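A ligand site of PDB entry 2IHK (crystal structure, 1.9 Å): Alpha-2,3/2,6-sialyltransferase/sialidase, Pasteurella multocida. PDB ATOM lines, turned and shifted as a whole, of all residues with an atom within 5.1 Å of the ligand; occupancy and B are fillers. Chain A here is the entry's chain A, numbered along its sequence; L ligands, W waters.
Residues that only touch the ligand: Thr 244 (3.5 Å), Ile 311 (3.5 Å), Leu 13 (3.5 Å), Gly 118 (3.6 Å), Pro 288 (3.6 Å), Leu 333 (3.6 Å), Ser 331 (3.7 Å), Ser 12 (3.7 Å) and Thr 241 (3.9 Å). Hydrophobic or aromatic side chains within 4 Å of the ligand: Leu 13, Met 120, Trp 246, His 287, Pro 288, Phe 313 and Leu 333. Of the 30 residues printed, 22 come within 4 Å of the ligand. Along chain A the residues within 4 Å of the ligand span positions 12 to 333.
The backbone NH (N) of Ser 119 is in hydrogen-bond range of the side-chain hydroxyl (OG) of Ser 332, 2.9 Å away. NH1 of Arg 39 is in hydrogen-bond range of OG of Ser 12. The backbone carbonyl oxygen (O) of Ala 309 is in hydrogen-bond range of the side-chain amino group (NZ) of Lys 285 (2.9 Å). N of Ser 331 sits close to OH of Tyr 364 (3.4 Å). The backbone carbonyl oxygen (O) of Lys 285 is in hydrogen-bond range of the backbone NH (N) of Gly 242. The side-chain carboxylate of Glu 121 sits at hydrogen-bond distance from the backbone NH of Asp 117. The side-chain amino group (NZ) of Lys 285 sits at hydrogen-bond distance from the backbone carbonyl oxygen (O) of Ile 311. N of Leu 333 lies close to OG of Ser 331 (3.4 Å).
Water W6 lies within hydrogen-bond range of OG of Ser 119 (2.7 Å), O9 of the ligand (2.7 Å) and OH of Tyr 364 (2.7 Å). Water W3 lies within hydrogen-bond range of the side-chain hydroxyl (OG1) of Thr 243 (2.6 Å), an oxygen (O4) of the ligand (2.8 Å) and the backbone carbonyl oxygen (O) of Ala 330 (2.8 Å). Water W4 lies within hydrogen-bond range of O of Asp 117 (2.6 Å), O6 of the ligand (2.9 Å), N of Ser 12 (3.1 Å) and N of Leu 13 (3.1 Å). Water W5 bridges the side-chain hydroxyl (OG1) of Thr 243 (2.8 Å) and an oxygen (O3) of the ligand (3.1 Å).
The backbone NH (N) of Ser 332 lies within hydrogen-bond range of an oxygen (O9) of the ligand (2.8 Å). A nitrogen (N4) of the ligand sits at hydrogen-bond distance from the backbone carbonyl oxygen (O) of Gly 286, 3.5 Å away. O2 of the ligand is in hydrogen-bond range of N of Ser 119, 3.5 Å away. The side-chain carboxylate of Asp 117 sits at hydrogen-bond distance from an oxygen (O2) of the ligand, 2.7 Å away. The indole nitrogen (NE1) of Trp 246 lies within hydrogen-bond range of an oxygen (O5) of the ligand, 2.7 Å away. N of Met 120 is in hydrogen-bond range of O2 of the ligand, 2.9 Å away. OG of Ser 312 sits at hydrogen-bond distance from O13 of the ligand, at 2.9 Å. An oxygen (O14) of the ligand is in hydrogen-bond range of the side-chain amino group (NZ) of Lys 285 (3.0 Å). NE2 of His 287 sits at hydrogen-bond distance from O15 of the ligand (2.6 Å). The side-chain hydroxyl (OG) of Ser 119 lies within hydrogen-bond range of a nitrogen (N1) of the ligand (2.9 Å). O7 of the ligand is in salt-bridge range of NH2 of Arg 39 (2.8 Å). O14 of the ligand sits at hydrogen-bond distance from N of Phe 313, at 2.8 Å. The backbone carbonyl oxygen of Gly 242 sits at hydrogen-bond distance from a nitrogen (N4) of the ligand (2.9 Å). The side-chain hydroxyl (OG) of Ser 332 is in hydrogen-bond range of an oxygen (O9) of the ligand. The backbone carbonyl oxygen of Lys 285 sits at hydrogen-bond distance from a nitrogen (N4) of the ligand (2.9 Å). The side-chain carboxylate (OE2) of Glu 314 lies within hydrogen-bond range of an oxygen (O13) of the ligand (2.5 Å).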
ATOM      1  N   ALA A  11      16.253   0.946 -27.196  1.00  0.00           N
ATOM      2  CA  ALA A  11      15.640  -0.369 -27.083  1.00  0.00           C
ATOM      3  C   ALA A  11      16.557  -1.444 -26.445  1.00  0.00           C
ATOM      4  O   ALA A  11      17.295  -1.136 -25.497  1.00  0.00           O
ATOM      5  CB  ALA A  11      15.091  -0.797 -28.467  1.00  0.00           C
ATOM      6  N   SER A  12      16.523  -2.679 -26.943  1.00  0.00           N
ATOM      7  CA  SER A  12      17.297  -3.794 -26.355  1.00  0.00           C
ATOM      8  C   SER A  12      18.347  -4.401 -27.265  1.00  0.00           C
ATOM      9  O   SER A  12      19.516  -4.563 -26.867  1.00  0.00           O
ATOM     10  CB  SER A  12      16.364  -4.904 -25.845  1.00  0.00           C
ATOM     11  OG  SER A  12      15.584  -4.463 -24.745  1.00  0.00           O
ATOM     12  N   LEU A  13      17.940  -4.808 -28.469  1.00  0.00           N
ATOM     13  CA  LEU A  13      18.821  -5.581 -29.347  1.00  0.00           C
ATOM     14  C   LEU A  13      20.056  -4.799 -29.803  1.00  0.00           C
ATOM     15  O   LEU A  13      21.165  -5.344 -29.774  1.00  0.00           O
ATOM     16  CB  LEU A  13      18.009  -6.126 -30.548  1.00  0.00           C
ATOM     17  CG  LEU A  13      17.913  -7.602 -30.920  1.00  0.00           C
ATOM     18  CD1 LEU A  13      18.314  -8.586 -29.831  1.00  0.00           C
ATOM     19  CD2 LEU A  13      16.501  -7.915 -31.473  1.00  0.00           C
ATOM     20  N   LEU A  16      22.412  -4.623 -26.804  1.00  0.00           N
ATOM     21  CA  LEU A  16      23.045  -5.906 -26.534  1.00  0.00           C
ATOM     22  C   LEU A  16      24.285  -6.108 -27.415  1.00  0.00           C
ATOM     23  O   LEU A  16      25.346  -6.472 -26.910  1.00  0.00           O
ATOM     24  CB  LEU A  16      21.994  -7.013 -26.701  1.00  0.00           C
ATOM     25  CG  LEU A  16      21.893  -8.244 -25.829  1.00  0.00           C
ATOM     26  CD1 LEU A  16      21.750  -7.877 -24.349  1.00  0.00           C
ATOM     27  CD2 LEU A  16      20.712  -9.070 -26.352  1.00  0.00           C
ATOM     28  N   ARG A  39      17.917   1.190 -21.714  1.00  0.00           N
ATOM     29  CA  ARG A  39      17.515  -0.019 -20.998  1.00  0.00           C
ATOM     30  C   ARG A  39      18.660  -0.680 -20.240  1.00  0.00           C
ATOM     31  O   ARG A  39      18.480  -1.775 -19.677  1.00  0.00           O
ATOM     32  CB  ARG A  39      16.885  -1.023 -21.983  1.00  0.00           C
ATOM     33  CG  ARG A  39      15.593  -0.511 -22.619  1.00  0.00           C
ATOM     34  CD  ARG A  39      14.783  -1.628 -23.237  1.00  0.00           C
ATOM     35  NE  ARG A  39      13.632  -1.099 -23.977  1.00  0.00           N
ATOM     36  CZ  ARG A  39      12.944  -1.760 -24.900  1.00  0.00           C
ATOM     37  NH1 ARG A  39      13.252  -3.024 -25.213  1.00  0.00           N
ATOM     38  NH2 ARG A  39      11.910  -1.171 -25.500  1.00  0.00           N
ATOM     39  N   ASP A 117      16.594  -2.610 -34.359  1.00  0.00           N
ATOM     40  CA  ASP A 117      15.695  -2.483 -33.208  1.00  0.00           C
ATOM     41  C   ASP A 117      15.159  -3.880 -32.865  1.00  0.00           C
ATOM     42  O   ASP A 117      15.201  -4.332 -31.706  1.00  0.00           O
ATOM     43  CB  ASP A 117      14.562  -1.503 -33.631  1.00  0.00           C
ATOM     44  CG  ASP A 117      13.596  -1.115 -32.507  1.00  0.00           C
ATOM     45  OD1 ASP A 117      14.012  -0.428 -31.520  1.00  0.00           O
ATOM     46  OD2 ASP A 117      12.390  -1.385 -32.662  1.00  0.00           O
ATOM     47  N   GLY A 118      14.650  -4.553 -33.903  1.00  0.00           N
ATOM     48  CA  GLY A 118      14.156  -5.941 -33.804  1.00  0.00           C
ATOM     49  C   GLY A 118      13.176  -6.253 -34.926  1.00  0.00           C
ATOM     50  O   GLY A 118      13.457  -5.975 -36.116  1.00  0.00           O
ATOM     51  N   SER A 119      12.010  -6.803 -34.566  1.00  0.00           N
ATOM     52  CA  SER A 119      10.983  -7.133 -35.550  1.00  0.00           C
ATOM     53  C   SER A 119      10.429  -5.926 -36.318  1.00  0.00           C
ATOM     54  O   SER A 119       9.964  -6.095 -37.452  1.00  0.00           O
ATOM     55  CB  SER A 119       9.824  -7.857 -34.910  1.00  0.00           C
ATOM     56  OG  SER A 119       9.234  -7.050 -33.897  1.00  0.00           O
ATOM     57  N   MET A 120      10.441  -4.738 -35.713  1.00  0.00           N
ATOM     58  CA  MET A 120       9.858  -3.568 -36.390  1.00  0.00           C
ATOM     59  C   MET A 120      10.430  -3.288 -37.776  1.00  0.00           C
ATOM     60  O   MET A 120       9.654  -2.985 -38.698  1.00  0.00           O
ATOM     61  CB  MET A 120       9.929  -2.286 -35.556  1.00  0.00           C
ATOM     62  CG  MET A 120       9.166  -1.147 -36.261  1.00  0.00           C
ATOM     63  SD  MET A 120       8.759   0.265 -35.225  1.00  0.00           S
ATOM     64  CE  MET A 120      10.339   1.011 -35.117  1.00  0.00           C
ATOM     65  N   GLU A 121      11.749  -3.394 -37.936  1.00  0.00           N
ATOM     66  CA  GLU A 121      12.370  -3.192 -39.255  1.00  0.00           C
ATOM     67  C   GLU A 121      11.758  -4.112 -40.295  1.00  0.00           C
ATOM     68  O   GLU A 121      11.512  -3.682 -41.426  1.00  0.00           O
ATOM     69  CB  GLU A 121      13.888  -3.358 -39.225  1.00  0.00           C
ATOM     70  CG  GLU A 121      14.647  -2.141 -38.684  1.00  0.00           C
ATOM     71  CD  GLU A 121      14.795  -2.167 -37.163  1.00  0.00           C
ATOM     72  OE1 GLU A 121      14.108  -3.000 -36.529  1.00  0.00           O
ATOM     73  OE2 GLU A 121      15.608  -1.375 -36.609  1.00  0.00           O
ATOM     74  N   VAL A 123       8.730  -5.909 -40.157  1.00  0.00           N
ATOM     75  CA  VAL A 123       7.308  -5.612 -40.364  1.00  0.00           C
ATOM     76  C   VAL A 123       7.180  -4.369 -41.277  1.00  0.00           C
ATOM     77  O   VAL A 123       6.345  -4.351 -42.182  1.00  0.00           O
ATOM     78  CB  VAL A 123       6.610  -5.442 -38.993  1.00  0.00           C
ATOM     79  CG1 VAL A 123       5.186  -4.849 -39.168  1.00  0.00           C
ATOM     80  CG2 VAL A 123       6.551  -6.789 -38.256  1.00  0.00           C
ATOM     81  N   THR A 241       7.258 -16.346 -22.549  1.00  0.00           N
ATOM     82  CA  THR A 241       7.785 -15.029 -22.839  1.00  0.00           C
ATOM     83  C   THR A 241       6.666 -13.995 -22.898  1.00  0.00           C
ATOM     84  O   THR A 241       5.623 -14.200 -23.534  1.00  0.00           O
ATOM     85  CB  THR A 241       8.619 -14.999 -24.138  1.00  0.00           C
ATOM     86  OG1 THR A 241       7.752 -15.205 -25.255  1.00  0.00           O
ATOM     87  CG2 THR A 241       9.710 -16.070 -24.116  1.00  0.00           C
ATOM     88  N   GLY A 242       6.885 -12.877 -22.215  1.00  0.00           N
ATOM     89  CA  GLY A 242       5.899 -11.824 -22.207  1.00  0.00           C
ATOM     90  C   GLY A 242       6.031 -10.765 -23.285  1.00  0.00           C
ATOM     91  O   GLY A 242       7.058 -10.638 -23.979  1.00  0.00           O
ATOM     92  N   THR A 243       4.981  -9.967 -23.392  1.00  0.00           N
ATOM     93  CA  THR A 243       4.941  -8.866 -24.338  1.00  0.00           C
ATOM     94  C   THR A 243       4.552  -7.593 -23.582  1.00  0.00           C
ATOM     95  O   THR A 243       4.383  -7.589 -22.332  1.00  0.00           O
ATOM     96  CB  THR A 243       3.983  -9.167 -25.526  1.00  0.00           C
ATOM     97  OG1 THR A 243       4.217  -8.230 -26.603  1.00  0.00           O
ATOM     98  CG2 THR A 243       2.502  -9.117 -25.085  1.00  0.00           C
ATOM     99  N   THR A 244       4.474  -6.496 -24.320  1.00  0.00           N
ATOM    100  CA  THR A 244       3.957  -5.267 -23.728  1.00  0.00           C
ATOM    101  C   THR A 244       3.090  -4.502 -24.725  1.00  0.00           C
ATOM    102  O   THR A 244       2.990  -4.880 -25.907  1.00  0.00           O
ATOM    103  CB  THR A 244       5.112  -4.388 -23.183  1.00  0.00           C
ATOM    104  OG1 THR A 244       4.561  -3.370 -22.356  1.00  0.00           O
ATOM    105  CG2 THR A 244       5.927  -3.747 -24.349  1.00  0.00           C
ATOM    106  N   TRP A 246       2.634  -0.221 -25.818  1.00  0.00           N
ATOM    107  CA  TRP A 246       3.115   1.156 -25.609  1.00  0.00           C
ATOM    108  C   TRP A 246       2.000   2.123 -25.253  1.00  0.00           C
ATOM    109  O   TRP A 246       2.267   3.300 -24.964  1.00  0.00           O
ATOM    110  CB  TRP A 246       3.890   1.651 -26.856  1.00  0.00           C
ATOM    111  CG  TRP A 246       4.973   0.660 -27.201  1.00  0.00           C
ATOM    112  CD1 TRP A 246       5.093  -0.048 -28.357  1.00  0.00           C
ATOM    113  CD2 TRP A 246       6.031   0.230 -26.352  1.00  0.00           C
ATOM    114  NE1 TRP A 246       6.180  -0.880 -28.303  1.00  0.00           N
ATOM    115  CE2 TRP A 246       6.772  -0.740 -27.067  1.00  0.00           C
ATOM    116  CE3 TRP A 246       6.434   0.558 -25.045  1.00  0.00           C
ATOM    117  CZ2 TRP A 246       7.913  -1.366 -26.527  1.00  0.00           C
ATOM    118  CZ3 TRP A 246       7.563  -0.068 -24.513  1.00  0.00           C
ATOM    119  CH2 TRP A 246       8.277  -1.016 -25.252  1.00  0.00           C
ATOM    120  N   LYS A 285       9.678 -15.075 -18.541  1.00  0.00           N
ATOM    121  CA  LYS A 285      10.616 -14.074 -19.037  1.00  0.00           C
ATOM    122  C   LYS A 285       9.774 -12.903 -19.517  1.00  0.00           C
ATOM    123  O   LYS A 285       9.317 -12.880 -20.656  1.00  0.00           O
ATOM    124  CB  LYS A 285      11.512 -14.661 -20.133  1.00  0.00           C
ATOM    125  CG  LYS A 285      12.550 -13.724 -20.807  1.00  0.00           C
ATOM    126  CD  LYS A 285      13.644 -13.187 -19.844  1.00  0.00           C
ATOM    127  CE  LYS A 285      13.301 -11.753 -19.375  1.00  0.00           C
ATOM    128  NZ  LYS A 285      13.478 -10.690 -20.433  1.00  0.00           N
ATOM    129  N   GLY A 286       9.556 -11.919 -18.647  1.00  0.00           N
ATOM    130  CA  GLY A 286       8.714 -10.790 -19.001  1.00  0.00           C
ATOM    131  C   GLY A 286       9.396  -9.839 -19.979  1.00  0.00           C
ATOM    132  O   GLY A 286      10.636  -9.840 -20.109  1.00  0.00           O
ATOM    133  N   HIS A 287       8.589  -9.006 -20.636  1.00  0.00           N
ATOM    134  CA  HIS A 287       9.122  -7.958 -21.532  1.00  0.00           C
ATOM    135  C   HIS A 287       9.908  -6.947 -20.678  1.00  0.00           C
ATOM    136  O   HIS A 287       9.431  -6.558 -19.597  1.00  0.00           O
ATOM    137  CB  HIS A 287       8.009  -7.261 -22.345  1.00  0.00           C
ATOM    138  CG  HIS A 287       8.557  -6.422 -23.477  1.00  0.00           C
ATOM    139  ND1 HIS A 287       9.117  -5.188 -23.272  1.00  0.00           N
ATOM    140  CD2 HIS A 287       8.713  -6.704 -24.790  1.00  0.00           C
ATOM    141  CE1 HIS A 287       9.565  -4.712 -24.433  1.00  0.00           C
ATOM    142  NE2 HIS A 287       9.336  -5.623 -25.371  1.00  0.00           N
ATOM    143  N   PRO A 288      11.096  -6.497 -21.154  1.00  0.00           N
ATOM    144  CA  PRO A 288      11.889  -5.509 -20.383  1.00  0.00           C
ATOM    145  C   PRO A 288      11.082  -4.266 -19.996  1.00  0.00           C
ATOM    146  O   PRO A 288      11.340  -3.674 -18.923  1.00  0.00           O
ATOM    147  CB  PRO A 288      13.039  -5.149 -21.338  1.00  0.00           C
ATOM    148  CG  PRO A 288      13.113  -6.261 -22.318  1.00  0.00           C
ATOM    149  CD  PRO A 288      11.774  -6.900 -22.400  1.00  0.00           C
ATOM    150  N   ALA A 309      13.105  -9.354 -15.812  1.00  0.00           N
ATOM    151  CA  ALA A 309      12.657  -8.856 -17.114  1.00  0.00           C
ATOM    152  C   ALA A 309      13.704  -8.118 -17.911  1.00  0.00           C
ATOM    153  O   ALA A 309      13.674  -8.137 -19.157  1.00  0.00           O
ATOM    154  CB  ALA A 309      11.376  -7.992 -16.955  1.00  0.00           C
ATOM    155  N   ILE A 311      16.767  -8.899 -18.289  1.00  0.00           N
ATOM    156  CA  ILE A 311      17.732  -9.802 -18.895  1.00  0.00           C
ATOM    157  C   ILE A 311      17.234 -10.177 -20.279  1.00  0.00           C
ATOM    158  O   ILE A 311      16.197 -10.830 -20.407  1.00  0.00           O
ATOM    159  CB  ILE A 311      17.980 -11.077 -17.993  1.00  0.00           C
ATOM    160  CG1 ILE A 311      18.568 -10.663 -16.636  1.00  0.00           C
ATOM    161  CG2 ILE A 311      18.903 -12.066 -18.701  1.00  0.00           C
ATOM    162  CD1 ILE A 311      18.762 -11.823 -15.621  1.00  0.00           C
ATOM    163  N   SER A 312      17.938  -9.770 -21.321  1.00  0.00           N
ATOM    164  CA  SER A 312      17.496 -10.120 -22.688  1.00  0.00           C
ATOM    165  C   SER A 312      17.554 -11.617 -22.888  1.00  0.00           C
ATOM    166  O   SER A 312      18.534 -12.250 -22.524  1.00  0.00           O
ATOM    167  CB  SER A 312      18.341  -9.431 -23.747  1.00  0.00           C
ATOM    168  OG  SER A 312      17.831  -8.146 -24.033  1.00  0.00           O
ATOM    169  N   PHE A 313      16.499 -12.166 -23.479  1.00  0.00           N
ATOM    170  CA  PHE A 313      16.417 -13.589 -23.758  1.00  0.00           C
ATOM    171  C   PHE A 313      17.673 -14.182 -24.445  1.00  0.00           C
ATOM    172  O   PHE A 313      18.143 -15.303 -24.095  1.00  0.00           O
ATOM    173  CB  PHE A 313      15.139 -13.878 -24.588  1.00  0.00           C
ATOM    174  CG  PHE A 313      14.883 -15.349 -24.794  1.00  0.00           C
ATOM    175  CD1 PHE A 313      15.545 -16.058 -25.800  1.00  0.00           C
ATOM    176  CD2 PHE A 313      14.010 -16.041 -23.956  1.00  0.00           C
ATOM    177  CE1 PHE A 313      15.333 -17.419 -25.979  1.00  0.00           C
ATOM    178  CE2 PHE A 313      13.798 -17.402 -24.135  1.00  0.00           C
ATOM    179  CZ  PHE A 313      14.458 -18.088 -25.151  1.00  0.00           C
ATOM    180  N   GLU A 314      18.229 -13.457 -25.412  1.00  0.00           N
ATOM    181  CA  GLU A 314      19.381 -13.956 -26.181  1.00  0.00           C
ATOM    182  C   GLU A 314      20.623 -14.282 -25.334  1.00  0.00           C
ATOM    183  O   GLU A 314      21.491 -15.046 -25.764  1.00  0.00           O
ATOM    184  CB  GLU A 314      19.762 -12.984 -27.315  1.00  0.00           C
ATOM    185  CG  GLU A 314      18.665 -12.767 -28.378  1.00  0.00           C
ATOM    186  CD  GLU A 314      17.583 -11.766 -27.963  1.00  0.00           C
ATOM    187  OE1 GLU A 314      16.623 -11.607 -28.742  1.00  0.00           O
ATOM    188  OE2 GLU A 314      17.685 -11.137 -26.871  1.00  0.00           O
ATOM    189  N   ALA A 330       4.311 -13.174 -30.054  1.00  0.00           N
ATOM    190  CA  ALA A 330       5.370 -12.861 -31.037  1.00  0.00           C
ATOM    191  C   ALA A 330       6.290 -11.754 -30.541  1.00  0.00           C
ATOM    192  O   ALA A 330       5.825 -10.701 -30.090  1.00  0.00           O
ATOM    193  CB  ALA A 330       4.734 -12.480 -32.356  1.00  0.00           C
ATOM    194  N   SER A 331       7.599 -12.032 -30.592  1.00  0.00           N
ATOM    195  CA  SER A 331       8.642 -11.160 -30.052  1.00  0.00           C
ATOM    196  C   SER A 331       9.886 -11.324 -30.909  1.00  0.00           C
ATOM    197  O   SER A 331      10.065 -12.367 -31.557  1.00  0.00           O
ATOM    198  CB  SER A 331       8.956 -11.559 -28.597  1.00  0.00           C
ATOM    199  OG  SER A 331      10.107 -10.874 -28.140  1.00  0.00           O
ATOM    200  N   SER A 332      10.762 -10.319 -30.898  1.00  0.00           N
ATOM    201  CA  SER A 332      12.011 -10.394 -31.661  1.00  0.00           C
ATOM    202  C   SER A 332      12.894 -11.562 -31.210  1.00  0.00           C
ATOM    203  O   SER A 332      13.736 -12.038 -31.964  1.00  0.00           O
ATOM    204  CB  SER A 332      12.805  -9.078 -31.533  1.00  0.00           C
ATOM    205  OG  SER A 332      11.977  -7.972 -31.884  1.00  0.00           O
ATOM    206  N   LEU A 333      12.731 -12.022 -29.976  1.00  0.00           N
ATOM    207  CA  LEU A 333      13.551 -13.127 -29.454  1.00  0.00           C
ATOM    208  C   LEU A 333      13.356 -14.412 -30.272  1.00  0.00           C
ATOM    209  O   LEU A 333      14.279 -15.240 -30.359  1.00  0.00           O
ATOM    210  CB  LEU A 333      13.280 -13.351 -27.937  1.00  0.00           C
ATOM    211  CG  LEU A 333      11.915 -13.956 -27.574  1.00  0.00           C
ATOM    212  CD1 LEU A 333      11.970 -15.516 -27.545  1.00  0.00           C
ATOM    213  CD2 LEU A 333      11.505 -13.396 -26.216  1.00  0.00           C
ATOM    214  N   TYR A 364       3.323  -8.978 -39.612  1.00  0.00           N
ATOM    215  CA  TYR A 364       4.187  -9.705 -38.691  1.00  0.00           C
ATOM    216  C   TYR A 364       4.083 -11.213 -38.967  1.00  0.00           C
ATOM    217  O   TYR A 364       5.092 -11.923 -39.014  1.00  0.00           O
ATOM    218  CB  TYR A 364       3.830  -9.412 -37.228  1.00  0.00           C
ATOM    219  CG  TYR A 364       4.945  -9.623 -36.194  1.00  0.00           C
ATOM    220  CD1 TYR A 364       4.819  -9.091 -34.908  1.00  0.00           C
ATOM    221  CD2 TYR A 364       6.116 -10.313 -36.495  1.00  0.00           C
ATOM    222  CE1 TYR A 364       5.807  -9.252 -33.950  1.00  0.00           C
ATOM    223  CE2 TYR A 364       7.136 -10.492 -35.550  1.00  0.00           C
ATOM    224  CZ  TYR A 364       6.968  -9.968 -34.277  1.00  0.00           C
ATOM    225  OH  TYR A 364       7.964 -10.129 -33.348  1.00  0.00           O
HETATM  226  C1  LIG L   1       9.147  -3.777 -31.808  1.00  0.00           C
HETATM  227  C2  LIG L   1      10.631  -4.191 -31.900  1.00  0.00           C
HETATM  228  C3  LIG L   1      10.777  -4.190 -29.434  1.00  0.00           C
HETATM  229  O1  LIG L   1       9.360  -3.925 -29.394  1.00  0.00           O
HETATM  230  C4  LIG L   1       8.611  -4.424 -30.501  1.00  0.00           C
HETATM  231  C5  LIG L   1      11.342  -3.547 -30.704  1.00  0.00           C
HETATM  232  O2  LIG L   1      11.263  -3.763 -33.100  1.00  0.00           O
HETATM  233  N1  LIG L   1       8.415  -4.390 -32.922  1.00  0.00           N
HETATM  234  C6  LIG L   1       7.152  -4.120 -30.159  1.00  0.00           C
HETATM  235  C7  LIG L   1       6.772  -4.685 -28.780  1.00  0.00           C
HETATM  236  C8  LIG L   1       5.310  -4.415 -28.433  1.00  0.00           C
HETATM  237  O3  LIG L   1       4.525  -5.060 -29.442  1.00  0.00           O
HETATM  238  O4  LIG L   1       6.977  -6.104 -28.764  1.00  0.00           O
HETATM  239  O5  LIG L   1       6.968  -2.700 -30.196  1.00  0.00           O
HETATM  240  C9  LIG L   1      11.418  -3.542 -28.216  1.00  0.00           C
HETATM  241  O6  LIG L   1      12.420  -4.049 -27.727  1.00  0.00           O
HETATM  242  O7  LIG L   1      10.924  -2.495 -27.743  1.00  0.00           O
HETATM  243  O8  LIG L   1      11.125  -5.577 -29.553  1.00  0.00           O
HETATM  244  O9  LIG L   1      10.070  -7.740 -30.035  1.00  0.00           O
HETATM  245  N2  LIG L   1      12.912  -9.341 -24.765  1.00  0.00           N
HETATM  246  C10 LIG L   1      13.115 -10.264 -23.724  1.00  0.00           C
HETATM  247  N3  LIG L   1      12.067 -10.940 -23.206  1.00  0.00           N
HETATM  248  C11 LIG L   1      10.805 -10.722 -23.653  1.00  0.00           C
HETATM  249  C12 LIG L   1      10.585  -9.807 -24.679  1.00  0.00           C
HETATM  250  C13 LIG L   1      11.659  -9.120 -25.227  1.00  0.00           C
HETATM  251  C14 LIG L   1      14.254  -9.163 -27.574  1.00  0.00           C
HETATM  252  C15 LIG L   1      14.888  -9.535 -26.234  1.00  0.00           C
HETATM  253  C16 LIG L   1      14.092  -8.617 -25.298  1.00  0.00           C
HETATM  254  O10 LIG L   1      13.697  -7.494 -26.092  1.00  0.00           O
HETATM  255  C17 LIG L   1      14.132  -7.663 -27.445  1.00  0.00           C
HETATM  256  P1  LIG L   1      10.514  -6.906 -28.847  1.00  0.00           P
HETATM  257  O11 LIG L   1      11.829  -7.630 -28.246  1.00  0.00           O
HETATM  258  C18 LIG L   1      13.123  -7.032 -28.415  1.00  0.00           C
HETATM  259  O12 LIG L   1      15.066  -9.540 -28.698  1.00  0.00           O
HETATM  260  O13 LIG L   1      16.277  -9.163 -26.224  1.00  0.00           O
HETATM  261  N4  LIG L   1       9.766 -11.391 -23.122  1.00  0.00           N
HETATM  262  O14 LIG L   1      14.287 -10.473 -23.319  1.00  0.00           O
HETATM  263  O15 LIG L   1       9.545  -6.504 -27.789  1.00  0.00           O
HETATM  264  C19 LIG L   1       7.353  -3.836 -33.545  1.00  0.00           C
HETATM  265  O16 LIG L   1       6.893  -2.734 -33.244  1.00  0.00           O
HETATM  266  C20 LIG L   1       6.760  -4.680 -34.659  1.00  0.00           C
HETATM  267  F1  LIG L   1      12.710  -3.730 -30.784  1.00  0.00           F
HETATM  268  O   HOH W   1       9.896  -0.161 -29.254  1.00  0.00           O
HETATM  269  O   HOH W   2       3.123  -2.690 -30.668  1.00  0.00           O
HETATM  270  O   HOH W   3       6.287  -8.733 -28.169  1.00  0.00           O
HETATM  271  O   HOH W   4      14.982  -4.214 -29.137  1.00  0.00           O
HETATM  272  O   HOH W   5       2.620  -7.458 -28.804  1.00  0.00           O
HETATM  273  O   HOH W   6       7.962  -7.930 -31.730  1.00  0.00           O
HETATM  274  O   HOH W   7       5.310  -6.916 -31.345  1.00  0.00           O
